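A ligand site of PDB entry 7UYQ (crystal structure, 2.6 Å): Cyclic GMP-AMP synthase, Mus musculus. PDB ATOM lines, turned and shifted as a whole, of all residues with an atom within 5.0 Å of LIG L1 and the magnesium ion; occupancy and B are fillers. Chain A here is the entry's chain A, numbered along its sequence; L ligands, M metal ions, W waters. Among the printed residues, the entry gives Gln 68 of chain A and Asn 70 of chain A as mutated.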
ATOM      1  N   THR A  54      34.182 -17.031 -23.888  1.00  0.00           N
ATOM      2  CA  THR A  54      33.034 -16.226 -24.275  1.00  0.00           C
ATOM      3  C   THR A  54      33.117 -14.784 -23.790  1.00  0.00           C
ATOM      4  O   THR A  54      34.057 -14.401 -23.072  1.00  0.00           O
ATOM      5  CB  THR A  54      31.761 -16.876 -23.737  1.00  0.00           C
ATOM      6  OG1 THR A  54      31.921 -17.130 -22.359  1.00  0.00           O
ATOM      7  CG2 THR A  54      31.551 -18.189 -24.396  1.00  0.00           C
ATOM      8  N   GLY A  55      32.141 -13.979 -24.224  1.00  0.00           N
ATOM      9  CA  GLY A  55      32.004 -12.622 -23.740  1.00  0.00           C
ATOM     10  C   GLY A  55      32.961 -11.633 -24.377  1.00  0.00           C
ATOM     11  O   GLY A  55      33.636 -11.951 -25.378  1.00  0.00           O
ATOM     12  N   SER A  56      33.055 -10.442 -23.777  1.00  0.00           N
ATOM     13  CA  SER A  56      33.583  -9.267 -24.453  1.00  0.00           C
ATOM     14  C   SER A  56      35.039  -9.414 -24.856  1.00  0.00           C
ATOM     15  O   SER A  56      35.417  -8.997 -25.942  1.00  0.00           O
ATOM     16  CB  SER A  56      33.355  -7.996 -23.622  1.00  0.00           C
ATOM     17  OG  SER A  56      33.774  -8.137 -22.276  1.00  0.00           O
ATOM     18  N   GLN A  68      38.303  -8.496 -16.920  1.00  0.00           N
ATOM     19  CA  GLN A  68      37.133  -9.321 -16.745  1.00  0.00           C
ATOM     20  C   GLN A  68      37.023 -10.315 -17.911  1.00  0.00           C
ATOM     21  O   GLN A  68      36.862  -9.929 -19.060  1.00  0.00           O
ATOM     22  CB  GLN A  68      35.889  -8.448 -16.598  1.00  0.00           C
ATOM     23  CG  GLN A  68      34.740  -9.080 -15.848  1.00  0.00           C
ATOM     24  CD  GLN A  68      33.875  -9.999 -16.696  1.00  0.00           C
ATOM     25  OE1 GLN A  68      33.989 -10.051 -17.914  1.00  0.00           O
ATOM     26  NE2 GLN A  68      32.982 -10.713 -16.059  1.00  0.00           N
ATOM     27  N   ASN A  70      35.410 -14.189 -19.315  1.00  0.00           N
ATOM     28  CA  ASN A  70      34.298 -15.117 -19.190  1.00  0.00           C
ATOM     29  C   ASN A  70      34.644 -16.453 -19.831  1.00  0.00           C
ATOM     30  O   ASN A  70      35.049 -16.492 -21.002  1.00  0.00           O
ATOM     31  CB  ASN A  70      33.057 -14.540 -19.871  1.00  0.00           C
ATOM     32  CG  ASN A  70      32.647 -13.199 -19.275  1.00  0.00           C
ATOM     33  OD1 ASN A  70      31.997 -13.142 -18.231  1.00  0.00           O
ATOM     34  ND2 ASN A  70      33.033 -12.129 -19.922  1.00  0.00           N
ATOM     35  N   MET A  72      33.269 -20.606 -20.144  1.00  0.00           N
ATOM     36  CA  MET A  72      32.287 -21.654 -19.896  1.00  0.00           C
ATOM     37  C   MET A  72      32.994 -22.998 -19.836  1.00  0.00           C
ATOM     38  O   MET A  72      33.822 -23.312 -20.690  1.00  0.00           O
ATOM     39  CB  MET A  72      31.223 -21.665 -20.992  1.00  0.00           C
ATOM     40  CG  MET A  72      30.424 -20.373 -21.080  1.00  0.00           C
ATOM     41  SD  MET A  72      29.103 -20.365 -22.338  1.00  0.00           S
ATOM     42  CE  MET A  72      27.951 -21.546 -21.655  1.00  0.00           C
ATOM     43  N   PRO A 146      23.844 -14.967  -4.491  1.00  0.00           N
ATOM     44  CA  PRO A 146      22.743 -15.936  -4.626  1.00  0.00           C
ATOM     45  C   PRO A 146      22.030 -15.836  -5.982  1.00  0.00           C
ATOM     46  O   PRO A 146      21.900 -14.744  -6.492  1.00  0.00           O
ATOM     47  CB  PRO A 146      21.779 -15.557  -3.488  1.00  0.00           C
ATOM     48  CG  PRO A 146      22.629 -14.801  -2.498  1.00  0.00           C
ATOM     49  CD  PRO A 146      23.668 -14.081  -3.336  1.00  0.00           C
ATOM     50  N   GLY A 147      21.614 -16.983  -6.551  1.00  0.00           N
ATOM     51  CA  GLY A 147      20.995 -17.063  -7.856  1.00  0.00           C
ATOM     52  C   GLY A 147      21.914 -16.892  -9.076  1.00  0.00           C
ATOM     53  O   GLY A 147      21.490 -17.175 -10.186  1.00  0.00           O
ATOM     54  N   SER A 148      23.154 -16.416  -8.866  1.00  0.00           N
ATOM     55  CA  SER A 148      24.165 -16.282  -9.939  1.00  0.00           C
ATOM     56  C   SER A 148      24.719 -17.642 -10.381  1.00  0.00           C
ATOM     57  O   SER A 148      24.940 -18.532  -9.559  1.00  0.00           O
ATOM     58  CB  SER A 148      25.327 -15.390  -9.497  1.00  0.00           C
ATOM     59  OG  SER A 148      26.345 -15.334 -10.477  1.00  0.00           O
ATOM     60  N   PRO A 149      24.957 -17.845 -11.687  1.00  0.00           N
ATOM     61  CA  PRO A 149      25.523 -19.110 -12.176  1.00  0.00           C
ATOM     62  C   PRO A 149      27.052 -19.216 -12.054  1.00  0.00           C
ATOM     63  O   PRO A 149      27.600 -20.281 -12.309  1.00  0.00           O
ATOM     64  CB  PRO A 149      25.100 -19.083 -13.648  1.00  0.00           C
ATOM     65  CG  PRO A 149      25.143 -17.611 -14.013  1.00  0.00           C
ATOM     66  CD  PRO A 149      24.653 -16.897 -12.775  1.00  0.00           C
ATOM     67  N   ALA A 150      27.721 -18.113 -11.681  1.00  0.00           N
ATOM     68  CA  ALA A 150      29.153 -17.979 -11.847  1.00  0.00           C
ATOM     69  C   ALA A 150      29.929 -18.390 -10.606  1.00  0.00           C
ATOM     70  O   ALA A 150      29.487 -18.136  -9.493  1.00  0.00           O
ATOM     71  CB  ALA A 150      29.495 -16.547 -12.203  1.00  0.00           C
ATOM     72  N   ASP A 164      34.879 -15.030 -14.471  1.00  0.00           N
ATOM     73  CA  ASP A 164      33.597 -15.655 -14.210  1.00  0.00           C
ATOM     74  C   ASP A 164      33.574 -16.997 -14.891  1.00  0.00           C
ATOM     75  O   ASP A 164      33.533 -17.077 -16.125  1.00  0.00           O
ATOM     76  CB  ASP A 164      32.439 -14.805 -14.749  1.00  0.00           C
ATOM     77  CG  ASP A 164      32.124 -13.584 -13.879  1.00  0.00           C
ATOM     78  OD1 ASP A 164      32.694 -13.436 -12.771  1.00  0.00           O
ATOM     79  OD2 ASP A 164      31.270 -12.799 -14.325  1.00  0.00           O
ATOM     80  N   ILE A 166      31.660 -20.372 -15.675  1.00  0.00           N
ATOM     81  CA  ILE A 166      30.272 -20.779 -15.807  1.00  0.00           C
ATOM     82  C   ILE A 166      30.159 -22.246 -16.170  1.00  0.00           C
ATOM     83  O   ILE A 166      30.602 -22.658 -17.227  1.00  0.00           O
ATOM     84  CB  ILE A 166      29.533 -19.901 -16.846  1.00  0.00           C
ATOM     85  CG1 ILE A 166      29.117 -18.583 -16.201  1.00  0.00           C
ATOM     86  CG2 ILE A 166      28.244 -20.545 -17.324  1.00  0.00           C
ATOM     87  CD1 ILE A 166      30.288 -17.707 -15.837  1.00  0.00           C
ATOM     88  N   VAL A 205      22.783 -22.859 -18.207  1.00  0.00           N
ATOM     89  CA  VAL A 205      23.598 -22.453 -17.071  1.00  0.00           C
ATOM     90  C   VAL A 205      22.694 -22.386 -15.849  1.00  0.00           C
ATOM     91  O   VAL A 205      21.498 -22.136 -15.962  1.00  0.00           O
ATOM     92  CB  VAL A 205      24.285 -21.117 -17.325  1.00  0.00           C
ATOM     93  CG1 VAL A 205      25.162 -21.205 -18.570  1.00  0.00           C
ATOM     94  CG2 VAL A 205      23.278 -19.968 -17.464  1.00  0.00           C
ATOM     95  N   ARG A 221      18.931 -21.751 -16.997  1.00  0.00           N
ATOM     96  CA  ARG A 221      18.670 -20.682 -17.990  1.00  0.00           C
ATOM     97  C   ARG A 221      19.444 -20.998 -19.284  1.00  0.00           C
ATOM     98  O   ARG A 221      20.596 -21.464 -19.183  1.00  0.00           O
ATOM     99  CB  ARG A 221      19.094 -19.312 -17.446  1.00  0.00           C
ATOM    100  CG  ARG A 221      18.696 -18.141 -18.349  1.00  0.00           C
ATOM    101  CD  ARG A 221      19.137 -16.795 -17.814  1.00  0.00           C
ATOM    102  NE  ARG A 221      20.580 -16.624 -17.873  1.00  0.00           N
ATOM    103  CZ  ARG A 221      21.259 -15.689 -17.205  1.00  0.00           C
ATOM    104  NH1 ARG A 221      20.620 -14.825 -16.422  1.00  0.00           N
ATOM    105  NH2 ARG A 221      22.578 -15.617 -17.320  1.00  0.00           N
ATOM    106  N   LEU A 222      18.837 -20.734 -20.451  1.00  0.00           N
ATOM    107  CA  LEU A 222      19.486 -20.935 -21.727  1.00  0.00           C
ATOM    108  C   LEU A 222      20.611 -19.924 -21.877  1.00  0.00           C
ATOM    109  O   LEU A 222      20.487 -18.800 -21.446  1.00  0.00           O
ATOM    110  CB  LEU A 222      18.487 -20.763 -22.886  1.00  0.00           C
ATOM    111  CG  LEU A 222      17.478 -21.879 -23.104  1.00  0.00           C
ATOM    112  CD1 LEU A 222      16.281 -21.402 -23.911  1.00  0.00           C
ATOM    113  CD2 LEU A 222      18.127 -23.071 -23.785  1.00  0.00           C
ATOM    114  N   SER A 223      21.714 -20.359 -22.509  1.00  0.00           N
ATOM    115  CA  SER A 223      22.813 -19.469 -22.877  1.00  0.00           C
ATOM    116  C   SER A 223      23.131 -19.571 -24.365  1.00  0.00           C
ATOM    117  O   SER A 223      23.152 -20.674 -24.924  1.00  0.00           O
ATOM    118  CB  SER A 223      24.083 -19.822 -22.095  1.00  0.00           C
ATOM    119  OG  SER A 223      25.173 -19.014 -22.525  1.00  0.00           O
ATOM    120  N   PHE A 224      23.392 -18.413 -24.975  1.00  0.00           N
ATOM    121  CA  PHE A 224      23.715 -18.294 -26.401  1.00  0.00           C
ATOM    122  C   PHE A 224      25.049 -17.580 -26.606  1.00  0.00           C
ATOM    123  O   PHE A 224      25.253 -16.894 -27.598  1.00  0.00           O
ATOM    124  CB  PHE A 224      22.575 -17.562 -27.106  1.00  0.00           C
ATOM    125  CG  PHE A 224      21.266 -18.271 -26.992  1.00  0.00           C
ATOM    126  CD1 PHE A 224      21.007 -19.367 -27.787  1.00  0.00           C
ATOM    127  CD2 PHE A 224      20.339 -17.896 -26.058  1.00  0.00           C
ATOM    128  CE1 PHE A 224      19.812 -20.050 -27.683  1.00  0.00           C
ATOM    129  CE2 PHE A 224      19.126 -18.581 -25.926  1.00  0.00           C
ATOM    130  CZ  PHE A 224      18.871 -19.657 -26.753  1.00  0.00           C
ATOM    131  N   SER A 225      25.966 -17.742 -25.651  1.00  0.00           N
ATOM    132  CA  SER A 225      27.233 -17.035 -25.681  1.00  0.00           C
ATOM    133  C   SER A 225      28.074 -17.436 -26.861  1.00  0.00           C
ATOM    134  O   SER A 225      28.857 -16.636 -27.344  1.00  0.00           O
ATOM    135  CB  SER A 225      28.017 -17.286 -24.404  1.00  0.00           C
ATOM    136  OG  SER A 225      27.324 -16.736 -23.305  1.00  0.00           O
ATOM    137  N   ASP A 273      21.623  -0.359 -10.739  1.00  0.00           N
ATOM    138  CA  ASP A 273      22.072  -1.726 -10.431  1.00  0.00           C
ATOM    139  C   ASP A 273      21.340  -2.811 -11.223  1.00  0.00           C
ATOM    140  O   ASP A 273      21.914  -3.852 -11.513  1.00  0.00           O
ATOM    141  CB  ASP A 273      21.989  -2.026  -8.927  1.00  0.00           C
ATOM    142  CG  ASP A 273      23.184  -1.468  -8.141  1.00  0.00           C
ATOM    143  OD1 ASP A 273      24.258  -1.226  -8.732  1.00  0.00           O
ATOM    144  OD2 ASP A 273      23.055  -1.294  -6.903  1.00  0.00           O
ATOM    145  N   CYS A 276      22.757  -3.994 -16.974  1.00  0.00           N
ATOM    146  CA  CYS A 276      24.002  -4.701 -17.226  1.00  0.00           C
ATOM    147  C   CYS A 276      24.351  -4.570 -18.706  1.00  0.00           C
ATOM    148  O   CYS A 276      23.506  -4.222 -19.546  1.00  0.00           O
ATOM    149  CB  CYS A 276      23.900  -6.170 -16.824  1.00  0.00           C
ATOM    150  SG  CYS A 276      22.743  -7.172 -17.809  1.00  0.00           S
HETATM  151  P1  LIG L   1      22.898  -9.760 -12.266  1.00  0.00           P
HETATM  152  O1  LIG L   1      24.376 -10.091 -12.412  1.00  0.00           O
HETATM  153  O2  LIG L   1      22.218  -9.545 -13.600  1.00  0.00           O
HETATM  154  O3  LIG L   1      22.653  -8.618 -11.317  1.00  0.00           O
HETATM  155  O4  LIG L   1      22.174 -11.056 -11.608  1.00  0.00           O
HETATM  156  P2  LIG L   1      22.477 -12.628 -11.547  1.00  0.00           P
HETATM  157  O5  LIG L   1      22.998 -12.979 -10.190  1.00  0.00           O
HETATM  158  O6  LIG L   1      21.312 -13.381 -12.101  1.00  0.00           O
HETATM  159  O7  LIG L   1      23.695 -12.734 -12.589  1.00  0.00           O
HETATM  160  P3  LIG L   1      23.794 -12.836 -14.181  1.00  0.00           P
HETATM  161  O8  LIG L   1      22.633 -13.622 -14.687  1.00  0.00           O
HETATM  162  O9  LIG L   1      24.034 -11.485 -14.747  1.00  0.00           O
HETATM  163  O10 LIG L   1      25.134 -13.706 -14.326  1.00  0.00           O
HETATM  164  C1  LIG L   1      26.308 -13.312 -13.578  1.00  0.00           C
HETATM  165  C2  LIG L   1      27.520 -13.374 -14.465  1.00  0.00           C
HETATM  166  O11 LIG L   1      27.713 -14.734 -14.915  1.00  0.00           O
HETATM  167  C3  LIG L   1      27.451 -12.566 -15.767  1.00  0.00           C
HETATM  168  O12 LIG L   1      27.762 -11.190 -15.570  1.00  0.00           O
HETATM  169  C4  LIG L   1      28.502 -13.288 -16.606  1.00  0.00           C
HETATM  170  O13 LIG L   1      29.825 -12.934 -16.253  1.00  0.00           O
HETATM  171  C5  LIG L   1      28.212 -14.746 -16.239  1.00  0.00           C
HETATM  172  N1  LIG L   1      27.232 -15.370 -17.109  1.00  0.00           N
HETATM  173  C6  LIG L   1      25.874 -15.418 -16.928  1.00  0.00           C
HETATM  174  N2  LIG L   1      25.239 -16.042 -17.890  1.00  0.00           N
HETATM  175  C7  LIG L   1      26.248 -16.413 -18.770  1.00  0.00           C
HETATM  176  C8  LIG L   1      26.167 -17.113 -20.011  1.00  0.00           C
HETATM  177  O14 LIG L   1      25.154 -17.518 -20.580  1.00  0.00           O
HETATM  178  N3  LIG L   1      27.427 -17.278 -20.590  1.00  0.00           N
HETATM  179  C9  LIG L   1      28.620 -16.844 -20.038  1.00  0.00           C
HETATM  180  N4  LIG L   1      29.739 -17.100 -20.737  1.00  0.00           N
HETATM  181  N5  LIG L   1      28.696 -16.187 -18.875  1.00  0.00           N
HETATM  182  C10 LIG L   1      27.480 -16.013 -18.304  1.00  0.00           C
HETATM  183  P1  LG2 L   2      31.544  -7.081 -20.205  1.00  0.00           P
HETATM  184  O1  LG2 L   2      32.101  -8.171 -19.340  1.00  0.00           O
HETATM  185  O2  LG2 L   2      32.632  -6.266 -20.863  1.00  0.00           O
HETATM  186  O3  LG2 L   2      30.524  -6.226 -19.480  1.00  0.00           O
HETATM  187  O4  LG2 L   2      30.720  -7.810 -21.399  1.00  0.00           O
HETATM  188  P2  LG2 L   2      30.223  -9.320 -21.485  1.00  0.00           P
HETATM  189  O5  LG2 L   2      29.258  -9.495 -22.615  1.00  0.00           O
HETATM  190  O6  LG2 L   2      31.432 -10.198 -21.424  1.00  0.00           O
HETATM  191  O7  LG2 L   2      29.404  -9.406 -20.114  1.00  0.00           O
HETATM  192  P3  LG2 L   2      29.367 -10.411 -18.866  1.00  0.00           P
HETATM  193  O8  LG2 L   2      30.787 -10.725 -18.507  1.00  0.00           O
HETATM  194  O9  LG2 L   2      28.470  -9.834 -17.830  1.00  0.00           O
HETATM  195  O10 LG2 L   2      28.664 -11.710 -19.483  1.00  0.00           O
HETATM  196  C1  LG2 L   2      29.392 -12.663 -20.304  1.00  0.00           C
HETATM  197  C2  LG2 L   2      28.465 -13.266 -21.337  1.00  0.00           C
HETATM  198  O11 LG2 L   2      27.450 -14.061 -20.658  1.00  0.00           O
HETATM  199  C3  LG2 L   2      27.667 -12.287 -22.197  1.00  0.00           C
HETATM  200  O12 LG2 L   2      28.403 -11.858 -23.337  1.00  0.00           O
HETATM  201  C4  LG2 L   2      26.455 -13.143 -22.590  1.00  0.00           C
HETATM  202  O13 LG2 L   2      26.728 -14.021 -23.649  1.00  0.00           O
HETATM  203  C5  LG2 L   2      26.204 -13.901 -21.290  1.00  0.00           C
HETATM  204  N1  LG2 L   2      25.283 -13.232 -20.374  1.00  0.00           N
HETATM  205  C6  LG2 L   2      25.603 -12.310 -19.412  1.00  0.00           C
HETATM  206  N2  LG2 L   2      24.561 -11.872 -18.740  1.00  0.00           N
HETATM  207  C7  LG2 L   2      23.491 -12.543 -19.318  1.00  0.00           C
HETATM  208  C8  LG2 L   2      22.103 -12.482 -19.026  1.00  0.00           C
HETATM  209  O14 LG2 L   2      21.539 -11.778 -18.166  1.00  0.00           O
HETATM  210  N3  LG2 L   2      21.360 -13.324 -19.859  1.00  0.00           N
HETATM  211  C9  LG2 L   2      21.876 -14.128 -20.840  1.00  0.00           C
HETATM  212  N4  LG2 L   2      21.017 -14.878 -21.546  1.00  0.00           N
HETATM  213  N5  LG2 L   2      23.180 -14.192 -21.115  1.00  0.00           N
HETATM  214  C10 LG2 L   2      23.918 -13.385 -20.324  1.00  0.00           C
HETATM  215 MG    MG M   1      32.494  -9.855 -19.652  1.00  0.00          MG
HETATM  216  O   HOH W   1      19.882 -11.176 -12.554  1.00  0.00           O
HETATM  217  O   HOH W   2      24.204 -10.015 -16.949  1.00  0.00           O
HETATM  218  O   HOH W   3      22.379 -17.101 -19.590  1.00  0.00           O
HETATM  219  O   HOH W   4      34.624  -9.866 -20.592  1.00  0.00           O
HETATM  220  O   HOH W   5      31.371 -16.149 -17.934  1.00  0.00           O
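Residues that only touch the magnesium ion: Ser 56. Three residues have an atom within 4 Å of the magnesium ion: Ser 56, Gln 68 and Asn 70. The nearest printed residue that does not touch the magnesium ion is Gly 55 (5.0 Å).
An oxygen (O13) of LIG L1 sits at hydrogen-bond distance from the side-chain amide oxygen of Asn 70, 2.9 Å away. The side-chain carboxylate of Asp 164 lies within hydrogen-bond range of an oxygen (O13) of LIG L1, 2.4 Å away. An oxygen (O14) of LIG L1 is in hydrogen-bond range of the side-chain hydroxyl (OG) of Ser 223 (2.5 Å). N4 of LIG L1 lies within hydrogen-bond range of OG1 of Thr 54 (2.7 Å). The guanidinium group (NH1) of Arg 221 is in salt-bridge range of an oxygen (O8) of LIG L1, at 2.9 Å. The side-chain hydroxyl (OG) of Ser 225 lies within hydrogen-bond range of a nitrogen (N3) of LIG L1, at 2.8 Å. A nitrogen (N4) of LIG L1 sits close to the side-chain sulfur (SD) of Met 72, 3.7 Å away. The side-chain hydroxyl (OG) of Ser 225 lies within hydrogen-bond range of an oxygen (O13) of LG2 L2, 2.8 Å away. The backbone NH (N) of Ser 56 lies close to an oxygen (O6) of LG2 L2 (2.9 Å). O2 of LG2 L2 sits at hydrogen-bond distance from OG of Ser 56 (2.6 Å).
An oxygen (O12) of LIG L1 sits at hydrogen-bond distance from an oxygen (O9) of LG2 L2 (2.7 Å).
Water W4 lies within hydrogen-bond range of OG of Ser 56 (2.6 Å) and O of Gln 68 (2.7 Å). Water W2 lies within hydrogen-bond range of N2 of LG2 L2 (2.6 Å), O9 of LIG L1 (2.7 Å) and SG of Cys 276 (3.3 Å). Water W3 lies within hydrogen-bond range of the guanidinium group of Arg 221 (2.5 Å), an oxygen (O14) of LIG L1 (3.0 Å), the backbone carbonyl oxygen of Leu 222 (3.1 Å) and a nitrogen (N4) of LG2 L2 (3.3 Å).
The magnesium ion is bound by an oxygen (O1) of LG2 L2 (1.8 Å), an oxygen (O6) of LG2 L2 (2.1 Å), an oxygen (O8) of LG2 L2 (2.2 Å), the side-chain amide oxygen of Gln 68 (2.3 Å), water W4 (2.3 Å) and the side-chain amide nitrogen of Asn 70 (2.4 Å). The magnesium ion has six donor atoms within binding distance.
Ser 148 touches LIG L1 (CB to O5, 3.4 Å). CD of Pro 149 touches O10 of LIG L1, 3.6 Å away. Ala 150 touches LIG L1 (CB to O11, 3.7 Å). CG1 of Ile 166 touches N5 of LIG L1, 3.6 Å away. Of the 21 residues printed, 12 come within 4 Å of LIG L1. The nearest printed residue that does not touch LIG L1 is Val 205 (4.2 Å).
The side-chain amide nitrogen (NE2) of Gln 68 lies within hydrogen-bond range of the side-chain carboxylate (OD2) of Asp 164, 3.2 Å away. The backbone carbonyl oxygen (O) of Asn 70 lies within hydrogen-bond range of the backbone NH (N) of Thr 54 (3.1 Å). The side-chain hydroxyl of Ser 225 sits at hydrogen-bond distance from the side-chain hydroxyl of Ser 223, at 3.2 Å. The backbone carbonyl oxygen of Arg 221 lies within hydrogen-bond range of the backbone NH of Val 205 (2.8 Å). The side-chain hydroxyl of Ser 148 lies close to the backbone NH of Ala 150 (3.3 Å).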
